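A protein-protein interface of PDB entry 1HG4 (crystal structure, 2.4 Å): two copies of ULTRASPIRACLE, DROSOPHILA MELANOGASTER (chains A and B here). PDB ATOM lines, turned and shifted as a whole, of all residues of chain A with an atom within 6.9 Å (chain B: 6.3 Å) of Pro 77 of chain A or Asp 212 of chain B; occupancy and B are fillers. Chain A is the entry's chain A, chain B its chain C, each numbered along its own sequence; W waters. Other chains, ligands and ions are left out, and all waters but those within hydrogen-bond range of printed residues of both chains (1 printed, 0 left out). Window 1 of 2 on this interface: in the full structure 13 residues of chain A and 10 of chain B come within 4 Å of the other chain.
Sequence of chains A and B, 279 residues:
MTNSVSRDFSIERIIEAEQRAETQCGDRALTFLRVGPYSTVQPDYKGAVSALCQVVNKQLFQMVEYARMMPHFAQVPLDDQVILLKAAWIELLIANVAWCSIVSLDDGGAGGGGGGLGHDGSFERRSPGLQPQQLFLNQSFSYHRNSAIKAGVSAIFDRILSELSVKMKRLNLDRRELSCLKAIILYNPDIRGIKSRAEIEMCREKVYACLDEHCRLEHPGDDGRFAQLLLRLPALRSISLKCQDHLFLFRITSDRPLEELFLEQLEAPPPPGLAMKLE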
ATOM      1  N   PHE A  73      -7.575  18.005 -13.406  1.00  0.00           N
ATOM      2  CA  PHE A  73      -6.664  18.605 -14.382  1.00  0.00           C
ATOM      3  C   PHE A  73      -5.393  17.800 -14.637  1.00  0.00           C
ATOM      4  O   PHE A  73      -5.086  17.466 -15.781  1.00  0.00           O
ATOM      5  CB  PHE A  73      -6.262  20.014 -13.951  1.00  0.00           C
ATOM      6  CG  PHE A  73      -5.514  20.777 -15.013  1.00  0.00           C
ATOM      7  CD1 PHE A  73      -6.182  21.294 -16.120  1.00  0.00           C
ATOM      8  CD2 PHE A  73      -4.142  20.969 -14.917  1.00  0.00           C
ATOM      9  CE1 PHE A  73      -5.497  21.989 -17.108  1.00  0.00           C
ATOM     10  CE2 PHE A  73      -3.450  21.665 -15.909  1.00  0.00           C
ATOM     11  CZ  PHE A  73      -4.125  22.173 -16.999  1.00  0.00           C
ATOM     12  N   ALA A  74      -4.656  17.499 -13.572  1.00  0.00           N
ATOM     13  CA  ALA A  74      -3.405  16.746 -13.690  1.00  0.00           C
ATOM     14  C   ALA A  74      -3.606  15.327 -14.190  1.00  0.00           C
ATOM     15  O   ALA A  74      -2.634  14.618 -14.480  1.00  0.00           O
ATOM     16  CB  ALA A  74      -2.681  16.716 -12.347  1.00  0.00           C
ATOM     17  N   GLN A  75      -4.861  14.899 -14.295  1.00  0.00           N
ATOM     18  CA  GLN A  75      -5.124  13.557 -14.771  1.00  0.00           C
ATOM     19  C   GLN A  75      -5.232  13.446 -16.278  1.00  0.00           C
ATOM     20  O   GLN A  75      -4.839  12.437 -16.855  1.00  0.00           O
ATOM     21  CB  GLN A  75      -6.382  12.987 -14.124  1.00  0.00           C
ATOM     22  CG  GLN A  75      -6.079  12.241 -12.850  1.00  0.00           C
ATOM     23  CD  GLN A  75      -5.307  13.088 -11.869  1.00  0.00           C
ATOM     24  OE1 GLN A  75      -5.826  14.074 -11.332  1.00  0.00           O
ATOM     25  NE2 GLN A  75      -4.052  12.719 -11.631  1.00  0.00           N
ATOM     26  N   VAL A  76      -5.765  14.462 -16.930  1.00  0.00           N
ATOM     27  CA  VAL A  76      -5.877  14.370 -18.366  1.00  0.00           C
ATOM     28  C   VAL A  76      -4.466  14.285 -18.912  1.00  0.00           C
ATOM     29  O   VAL A  76      -3.509  14.672 -18.246  1.00  0.00           O
ATOM     30  CB  VAL A  76      -6.613  15.579 -18.953  1.00  0.00           C
ATOM     31  CG1 VAL A  76      -7.912  15.775 -18.206  1.00  0.00           C
ATOM     32  CG2 VAL A  76      -5.750  16.817 -18.888  1.00  0.00           C
ATOM     33  N   PRO A  77      -4.308  13.728 -20.116  1.00  0.00           N
ATOM     34  CA  PRO A  77      -2.942  13.647 -20.648  1.00  0.00           C
ATOM     35  C   PRO A  77      -2.283  15.027 -20.759  1.00  0.00           C
ATOM     36  O   PRO A  77      -2.948  16.036 -21.025  1.00  0.00           O
ATOM     37  CB  PRO A  77      -3.133  12.954 -22.004  1.00  0.00           C
ATOM     38  CG  PRO A  77      -4.587  13.216 -22.359  1.00  0.00           C
ATOM     39  CD  PRO A  77      -5.298  13.133 -21.034  1.00  0.00           C
ATOM     40  N   LEU A  78      -0.974  15.057 -20.528  1.00  0.00           N
ATOM     41  CA  LEU A  78      -0.181  16.284 -20.578  1.00  0.00           C
ATOM     42  C   LEU A  78      -0.493  17.132 -21.807  1.00  0.00           C
ATOM     43  O   LEU A  78      -0.658  18.344 -21.718  1.00  0.00           O
ATOM     44  CB  LEU A  78       1.303  15.931 -20.582  1.00  0.00           C
ATOM     45  CG  LEU A  78       2.129  16.483 -19.427  1.00  0.00           C
ATOM     46  CD1 LEU A  78       3.581  16.008 -19.552  1.00  0.00           C
ATOM     47  CD2 LEU A  78       2.042  18.008 -19.429  1.00  0.00           C
ATOM     48  N   ASP A  79      -0.574  16.489 -22.964  1.00  0.00           N
ATOM     49  CA  ASP A  79      -0.852  17.224 -24.182  1.00  0.00           C
ATOM     50  C   ASP A  79      -2.154  17.995 -24.060  1.00  0.00           C
ATOM     51  O   ASP A  79      -2.272  19.096 -24.579  1.00  0.00           O
ATOM     52  CB  ASP A  79      -0.870  16.279 -25.394  1.00  0.00           C
ATOM     53  CG  ASP A  79       0.513  15.684 -25.692  1.00  0.00           C
ATOM     54  OD1 ASP A  79       1.505  16.116 -25.058  1.00  0.00           O
ATOM     55  OD2 ASP A  79       0.621  14.786 -26.556  1.00  0.00           O
ATOM     56  N   ASP A  80      -3.126  17.432 -23.357  1.00  0.00           N
ATOM     57  CA  ASP A  80      -4.400  18.115 -23.191  1.00  0.00           C
ATOM     58  C   ASP A  80      -4.221  19.304 -22.251  1.00  0.00           C
ATOM     59  O   ASP A  80      -4.761  20.382 -22.501  1.00  0.00           O
ATOM     60  CB  ASP A  80      -5.470  17.175 -22.607  1.00  0.00           C
ATOM     61  CG  ASP A  80      -6.156  16.317 -23.662  1.00  0.00           C
ATOM     62  OD1 ASP A  80      -6.069  16.661 -24.862  1.00  0.00           O
ATOM     63  OD2 ASP A  80      -6.799  15.305 -23.283  1.00  0.00           O
ATOM     64  N   GLN A  81      -3.463  19.098 -21.175  1.00  0.00           N
ATOM     65  CA  GLN A  81      -3.233  20.136 -20.176  1.00  0.00           C
ATOM     66  C   GLN A  81      -2.623  21.377 -20.800  1.00  0.00           C
ATOM     67  O   GLN A  81      -2.978  22.508 -20.447  1.00  0.00           O
ATOM     68  CB  GLN A  81      -2.313  19.615 -19.073  1.00  0.00           C
ATOM     69  CG  GLN A  81      -2.905  18.489 -18.244  1.00  0.00           C
ATOM     70  CD  GLN A  81      -1.934  17.997 -17.196  1.00  0.00           C
ATOM     71  OE1 GLN A  81      -1.252  18.795 -16.549  1.00  0.00           O
ATOM     72  NE2 GLN A  81      -1.861  16.683 -17.019  1.00  0.00           N
ATOM     73  N   VAL A  82      -1.709  21.158 -21.735  1.00  0.00           N
ATOM     74  CA  VAL A  82      -1.030  22.246 -22.421  1.00  0.00           C
ATOM     75  C   VAL A  82      -2.013  23.029 -23.271  1.00  0.00           C
ATOM     76  O   VAL A  82      -1.981  24.256 -23.281  1.00  0.00           O
ATOM     77  CB  VAL A  82       0.128  21.697 -23.316  1.00  0.00           C
ATOM     78  CG1 VAL A  82       0.593  22.759 -24.304  1.00  0.00           C
ATOM     79  CG2 VAL A  82       1.284  21.246 -22.436  1.00  0.00           C
ATOM     80  N   LEU A  84      -5.314  23.276 -22.908  1.00  0.00           N
ATOM     81  CA  LEU A  84      -6.280  23.978 -22.064  1.00  0.00           C
ATOM     82  C   LEU A  84      -5.705  25.292 -21.572  1.00  0.00           C
ATOM     83  O   LEU A  84      -6.393  26.311 -21.586  1.00  0.00           O
ATOM     84  CB  LEU A  84      -6.681  23.106 -20.868  1.00  0.00           C
ATOM     85  CG  LEU A  84      -7.466  21.842 -21.238  1.00  0.00           C
ATOM     86  CD1 LEU A  84      -7.586  20.908 -20.045  1.00  0.00           C
ATOM     87  CD2 LEU A  84      -8.832  22.243 -21.746  1.00  0.00           C
ATOM     88  N   LYS A 195      -7.841  15.451 -26.410  1.00  0.00           N
ATOM     89  CA  LYS A 195      -8.122  14.027 -26.347  1.00  0.00           C
ATOM     90  C   LYS A 195      -9.288  13.680 -25.425  1.00  0.00           C
ATOM     91  O   LYS A 195     -10.228  12.993 -25.827  1.00  0.00           O
ATOM     92  CB  LYS A 195      -6.874  13.281 -25.873  1.00  0.00           C
ATOM     93  CG  LYS A 195      -6.329  12.273 -26.860  1.00  0.00           C
ATOM     94  CD  LYS A 195      -6.018  12.902 -28.206  1.00  0.00           C
ATOM     95  CE  LYS A 195      -5.558  11.839 -29.196  1.00  0.00           C
ATOM     96  NZ  LYS A 195      -5.469  12.345 -30.595  1.00  0.00           N
ATOM     97  N   SER A 196      -9.223  14.161 -24.190  1.00  0.00           N
ATOM     98  CA  SER A 196     -10.255  13.871 -23.202  1.00  0.00           C
ATOM     99  C   SER A 196     -11.423  14.861 -23.124  1.00  0.00           C
ATOM    100  O   SER A 196     -11.689  15.421 -22.070  1.00  0.00           O
ATOM    101  CB  SER A 196      -9.593  13.748 -21.837  1.00  0.00           C
ATOM    102  OG  SER A 196      -8.431  12.940 -21.939  1.00  0.00           O
ATOM    103  N   GLU B 205     -11.183   7.400 -22.614  1.00  0.00           N
ATOM    104  CA  GLU B 205     -10.430   8.497 -22.035  1.00  0.00           C
ATOM    105  C   GLU B 205      -9.676   8.078 -20.782  1.00  0.00           C
ATOM    106  O   GLU B 205      -8.600   8.589 -20.508  1.00  0.00           O
ATOM    107  CB  GLU B 205     -11.365   9.689 -21.790  1.00  0.00           C
ATOM    108  CG  GLU B 205     -11.793  10.342 -23.113  1.00  0.00           C
ATOM    109  CD  GLU B 205     -12.712  11.537 -22.940  1.00  0.00           C
ATOM    110  OE1 GLU B 205     -12.756  12.120 -21.840  1.00  0.00           O
ATOM    111  OE2 GLU B 205     -13.388  11.914 -23.910  1.00  0.00           O
ATOM    112  N   VAL B 207      -8.339   5.240 -20.425  1.00  0.00           N
ATOM    113  CA  VAL B 207      -7.191   4.490 -20.928  1.00  0.00           C
ATOM    114  C   VAL B 207      -6.137   5.500 -21.387  1.00  0.00           C
ATOM    115  O   VAL B 207      -4.933   5.272 -21.221  1.00  0.00           O
ATOM    116  CB  VAL B 207      -7.585   3.549 -22.106  1.00  0.00           C
ATOM    117  CG1 VAL B 207      -6.345   2.874 -22.676  1.00  0.00           C
ATOM    118  CG2 VAL B 207      -8.569   2.486 -21.622  1.00  0.00           C
ATOM    119  N   TYR B 208      -6.589   6.620 -21.956  1.00  0.00           N
ATOM    120  CA  TYR B 208      -5.667   7.676 -22.392  1.00  0.00           C
ATOM    121  C   TYR B 208      -4.871   8.119 -21.165  1.00  0.00           C
ATOM    122  O   TYR B 208      -3.634   8.231 -21.198  1.00  0.00           O
ATOM    123  CB  TYR B 208      -6.440   8.887 -22.927  1.00  0.00           C
ATOM    124  CG  TYR B 208      -6.949   8.775 -24.354  1.00  0.00           C
ATOM    125  CD1 TYR B 208      -6.315   7.962 -25.289  1.00  0.00           C
ATOM    126  CD2 TYR B 208      -8.059   9.508 -24.766  1.00  0.00           C
ATOM    127  CE1 TYR B 208      -6.776   7.888 -26.600  1.00  0.00           C
ATOM    128  CE2 TYR B 208      -8.530   9.435 -26.058  1.00  0.00           C
ATOM    129  CZ  TYR B 208      -7.892   8.625 -26.976  1.00  0.00           C
ATOM    130  OH  TYR B 208      -8.392   8.546 -28.258  1.00  0.00           O
ATOM    131  N   ALA B 209      -5.606   8.363 -20.080  1.00  0.00           N
ATOM    132  CA  ALA B 209      -5.016   8.805 -18.816  1.00  0.00           C
ATOM    133  C   ALA B 209      -4.015   7.792 -18.303  1.00  0.00           C
ATOM    134  O   ALA B 209      -2.990   8.168 -17.752  1.00  0.00           O
ATOM    135  CB  ALA B 209      -6.094   9.038 -17.780  1.00  0.00           C
ATOM    136  N   CYS B 210      -4.307   6.508 -18.487  1.00  0.00           N
ATOM    137  CA  CYS B 210      -3.387   5.450 -18.063  1.00  0.00           C
ATOM    138  C   CYS B 210      -2.145   5.423 -18.962  1.00  0.00           C
ATOM    139  O   CYS B 210      -1.019   5.351 -18.474  1.00  0.00           O
ATOM    140  CB  CYS B 210      -4.071   4.078 -18.118  1.00  0.00           C
ATOM    141  SG  CYS B 210      -5.244   3.784 -16.798  1.00  0.00           S
ATOM    142  N   LEU B 211      -2.360   5.473 -20.274  1.00  0.00           N
ATOM    143  CA  LEU B 211      -1.259   5.456 -21.227  1.00  0.00           C
ATOM    144  C   LEU B 211      -0.306   6.643 -20.988  1.00  0.00           C
ATOM    145  O   LEU B 211       0.923   6.468 -20.917  1.00  0.00           O
ATOM    146  CB  LEU B 211      -1.795   5.501 -22.661  1.00  0.00           C
ATOM    147  CG  LEU B 211      -0.743   5.360 -23.762  1.00  0.00           C
ATOM    148  CD1 LEU B 211       0.003   4.051 -23.579  1.00  0.00           C
ATOM    149  CD2 LEU B 211      -1.407   5.404 -25.131  1.00  0.00           C
ATOM    150  N   ASP B 212      -0.874   7.839 -20.845  1.00  0.00           N
ATOM    151  CA  ASP B 212      -0.067   9.037 -20.622  1.00  0.00           C
ATOM    152  C   ASP B 212       0.774   8.902 -19.357  1.00  0.00           C
ATOM    153  O   ASP B 212       1.971   9.194 -19.362  1.00  0.00           O
ATOM    154  CB  ASP B 212      -0.963  10.285 -20.520  1.00  0.00           C
ATOM    155  CG  ASP B 212      -0.163  11.590 -20.532  1.00  0.00           C
ATOM    156  OD1 ASP B 212       0.441  11.919 -21.572  1.00  0.00           O
ATOM    157  OD2 ASP B 212      -0.130  12.293 -19.500  1.00  0.00           O
ATOM    158  N   GLU B 213       0.146   8.455 -18.273  1.00  0.00           N
ATOM    159  CA  GLU B 213       0.851   8.283 -17.012  1.00  0.00           C
ATOM    160  C   GLU B 213       2.017   7.314 -17.174  1.00  0.00           C
ATOM    161  O   GLU B 213       3.126   7.558 -16.701  1.00  0.00           O
ATOM    162  CB  GLU B 213      -0.105   7.757 -15.948  1.00  0.00           C
ATOM    163  CG  GLU B 213       0.549   7.540 -14.598  1.00  0.00           C
ATOM    164  CD  GLU B 213      -0.408   6.989 -13.559  1.00  0.00           C
ATOM    165  OE1 GLU B 213      -1.046   5.947 -13.834  1.00  0.00           O
ATOM    166  OE2 GLU B 213      -0.521   7.594 -12.465  1.00  0.00           O
ATOM    167  N   HIS B 214       1.756   6.202 -17.841  1.00  0.00           N
ATOM    168  CA  HIS B 214       2.789   5.213 -18.054  1.00  0.00           C
ATOM    169  C   HIS B 214       3.955   5.941 -18.706  1.00  0.00           C
ATOM    170  O   HIS B 214       5.112   5.740 -18.336  1.00  0.00           O
ATOM    171  CB  HIS B 214       2.268   4.095 -18.967  1.00  0.00           C
ATOM    172  CG  HIS B 214       3.290   3.043 -19.283  1.00  0.00           C
ATOM    173  ND1 HIS B 214       3.704   2.101 -18.363  1.00  0.00           N
ATOM    174  CD2 HIS B 214       4.003   2.804 -20.410  1.00  0.00           C
ATOM    175  CE1 HIS B 214       4.627   1.331 -18.910  1.00  0.00           C
ATOM    176  NE2 HIS B 214       4.827   1.736 -20.151  1.00  0.00           N
ATOM    177  N   CYS B 215       3.640   6.809 -19.665  1.00  0.00           N
ATOM    178  CA  CYS B 215       4.669   7.563 -20.378  1.00  0.00           C
ATOM    179  C   CYS B 215       5.459   8.485 -19.469  1.00  0.00           C
ATOM    180  O   CYS B 215       6.683   8.396 -19.387  1.00  0.00           O
ATOM    181  CB  CYS B 215       4.047   8.374 -21.513  1.00  0.00           C
ATOM    182  SG  CYS B 215       3.790   7.429 -23.029  1.00  0.00           S
ATOM    183  N   ARG B 216       4.753   9.366 -18.777  1.00  0.00           N
ATOM    184  CA  ARG B 216       5.400  10.304 -17.878  1.00  0.00           C
ATOM    185  C   ARG B 216       6.274   9.621 -16.825  1.00  0.00           C
ATOM    186  O   ARG B 216       7.267  10.189 -16.376  1.00  0.00           O
ATOM    187  CB  ARG B 216       4.339  11.191 -17.223  1.00  0.00           C
ATOM    188  CG  ARG B 216       3.602  12.045 -18.242  1.00  0.00           C
ATOM    189  CD  ARG B 216       2.446  12.830 -17.634  1.00  0.00           C
ATOM    190  NE  ARG B 216       2.898  13.862 -16.707  1.00  0.00           N
ATOM    191  CZ  ARG B 216       2.085  14.724 -16.104  1.00  0.00           C
ATOM    192  NH1 ARG B 216       0.780  14.671 -16.333  1.00  0.00           N
ATOM    193  NH2 ARG B 216       2.576  15.634 -15.274  1.00  0.00           N
ATOM    194  N   LEU B 217       5.923   8.394 -16.457  1.00  0.00           N
ATOM    195  CA  LEU B 217       6.688   7.659 -15.455  1.00  0.00           C
ATOM    196  C   LEU B 217       7.835   6.803 -15.999  1.00  0.00           C
ATOM    197  O   LEU B 217       8.945   6.835 -15.463  1.00  0.00           O
ATOM    198  CB  LEU B 217       5.748   6.781 -14.634  1.00  0.00           C
ATOM    199  CG  LEU B 217       4.849   7.587 -13.704  1.00  0.00           C
ATOM    200  CD1 LEU B 217       3.827   6.674 -13.038  1.00  0.00           C
ATOM    201  CD2 LEU B 217       5.720   8.294 -12.664  1.00  0.00           C
ATOM    202  N   PHE B 226       3.604   9.849 -26.268  1.00  0.00           N
ATOM    203  CA  PHE B 226       2.170   9.590 -26.234  1.00  0.00           C
ATOM    204  C   PHE B 226       1.504   9.748 -27.599  1.00  0.00           C
ATOM    205  O   PHE B 226       0.803   8.857 -28.070  1.00  0.00           O
ATOM    206  CB  PHE B 226       1.508  10.529 -25.223  1.00  0.00           C
ATOM    207  CG  PHE B 226       0.011  10.371 -25.122  1.00  0.00           C
ATOM    208  CD1 PHE B 226      -0.552   9.352 -24.354  1.00  0.00           C
ATOM    209  CD2 PHE B 226      -0.839  11.258 -25.783  1.00  0.00           C
ATOM    210  CE1 PHE B 226      -1.934   9.223 -24.244  1.00  0.00           C
ATOM    211  CE2 PHE B 226      -2.226  11.138 -25.680  1.00  0.00           C
ATOM    212  CZ  PHE B 226      -2.776  10.116 -24.907  1.00  0.00           C
HETATM  213  O   HOH W   1       0.004  13.705 -23.569  1.00  0.00           O
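OD2 of Asp 212 of chain B lies within hydrogen-bond range of N of Leu 78 of chain A (3.1 Å). NH1 of Arg 216 of chain B sits close to NE2 of Gln 81 of chain A (3.4 Å). The backbone carbonyl oxygen (O) of Ser 196 of chain A lies close to the side-chain carboxylate (OE1) of Glu 205 of chain B (3.5 Å).
O of Ala 74 of chain A is in hydrogen-bond range of NE2 of Gln 81 of chain A, 3.4 Å away. O of Val 76 of chain A sits at hydrogen-bond distance from NE2 of Gln 81 of chain A, at 2.9 Å. The side-chain carboxylate (OD1) of Asp 80 of chain A is in hydrogen-bond range of the backbone NH (N) of Lys 195 of chain A (2.6 Å). OD2 of Asp 80 of chain A sits at hydrogen-bond distance from N of Ser 196 of chain A, 2.8 Å away.
Among the printed residues, merely in contact across the chains: Pro 77 of chain A with Asp 212 of chain B (3.3 Å), Leu 78 of chain A with Arg 216 of chain B (3.6 Å), Lys 195 of chain A with Tyr 208 of chain B (3.7 Å), Gln 75 of chain A with Ala 209 of chain B (3.7 Å), Lys 195 of chain A with Glu 205 of chain B (3.9 Å), Ala 74 of chain A with Arg 216 of chain B (3.9 Å) and Asp 79 of chain A with Phe 226 of chain B (3.9 Å).
Printed residues of chain B within 4 Å of Gln 75 of chain A: Ala 209. Val 76 of chain A touches none of the printed residues of chain B. Of chain B, only Asp 212 comes within 4 Å of Pro 77 of chain A. Printed residues of chain B within 4 Å of Gln 81 of chain A: Arg 216 (3.4 Å). Of the printed residues of chain B, Lys 195 of chain A touches Glu 205 (3.9 Å) and Tyr 208 (3.7 Å). Of chain A, only Pro 77 and Leu 78 come within 4 Å of Asp 212 of chain B. Cys 215 of chain B touches none of the printed residues of chain A. The nearest residue of chain A that does not touch Asp 212 of chain B is Val 76 of chain A (4.3 Å).
Hydrophobic or aromatic side chains of chain B within 4 Å of the printed part of chain A: Tyr 208, Ala 209 and Phe 226. Of the 13 printed residues of chain A, 8 touch a printed residue of chain B. Printed residues of chain A that touch a printed residue of chain B: Ala 74, Gln 75, Pro 77, Leu 78, Asp 79, Gln 81, Lys 195 and Ser 196. Among the printed residues, 10 pairs touch across the chains. Among the printed residues, no Asp or Glu carboxylate lies within 4 Å of a Lys or Arg side-chain nitrogen of the other chain.
No position is printed for both chains.
Water W1 lies within hydrogen-bond range of OD1 of Asp 212 of chain B, N of Asp 79 of chain A and N of Leu 78 of chain A.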
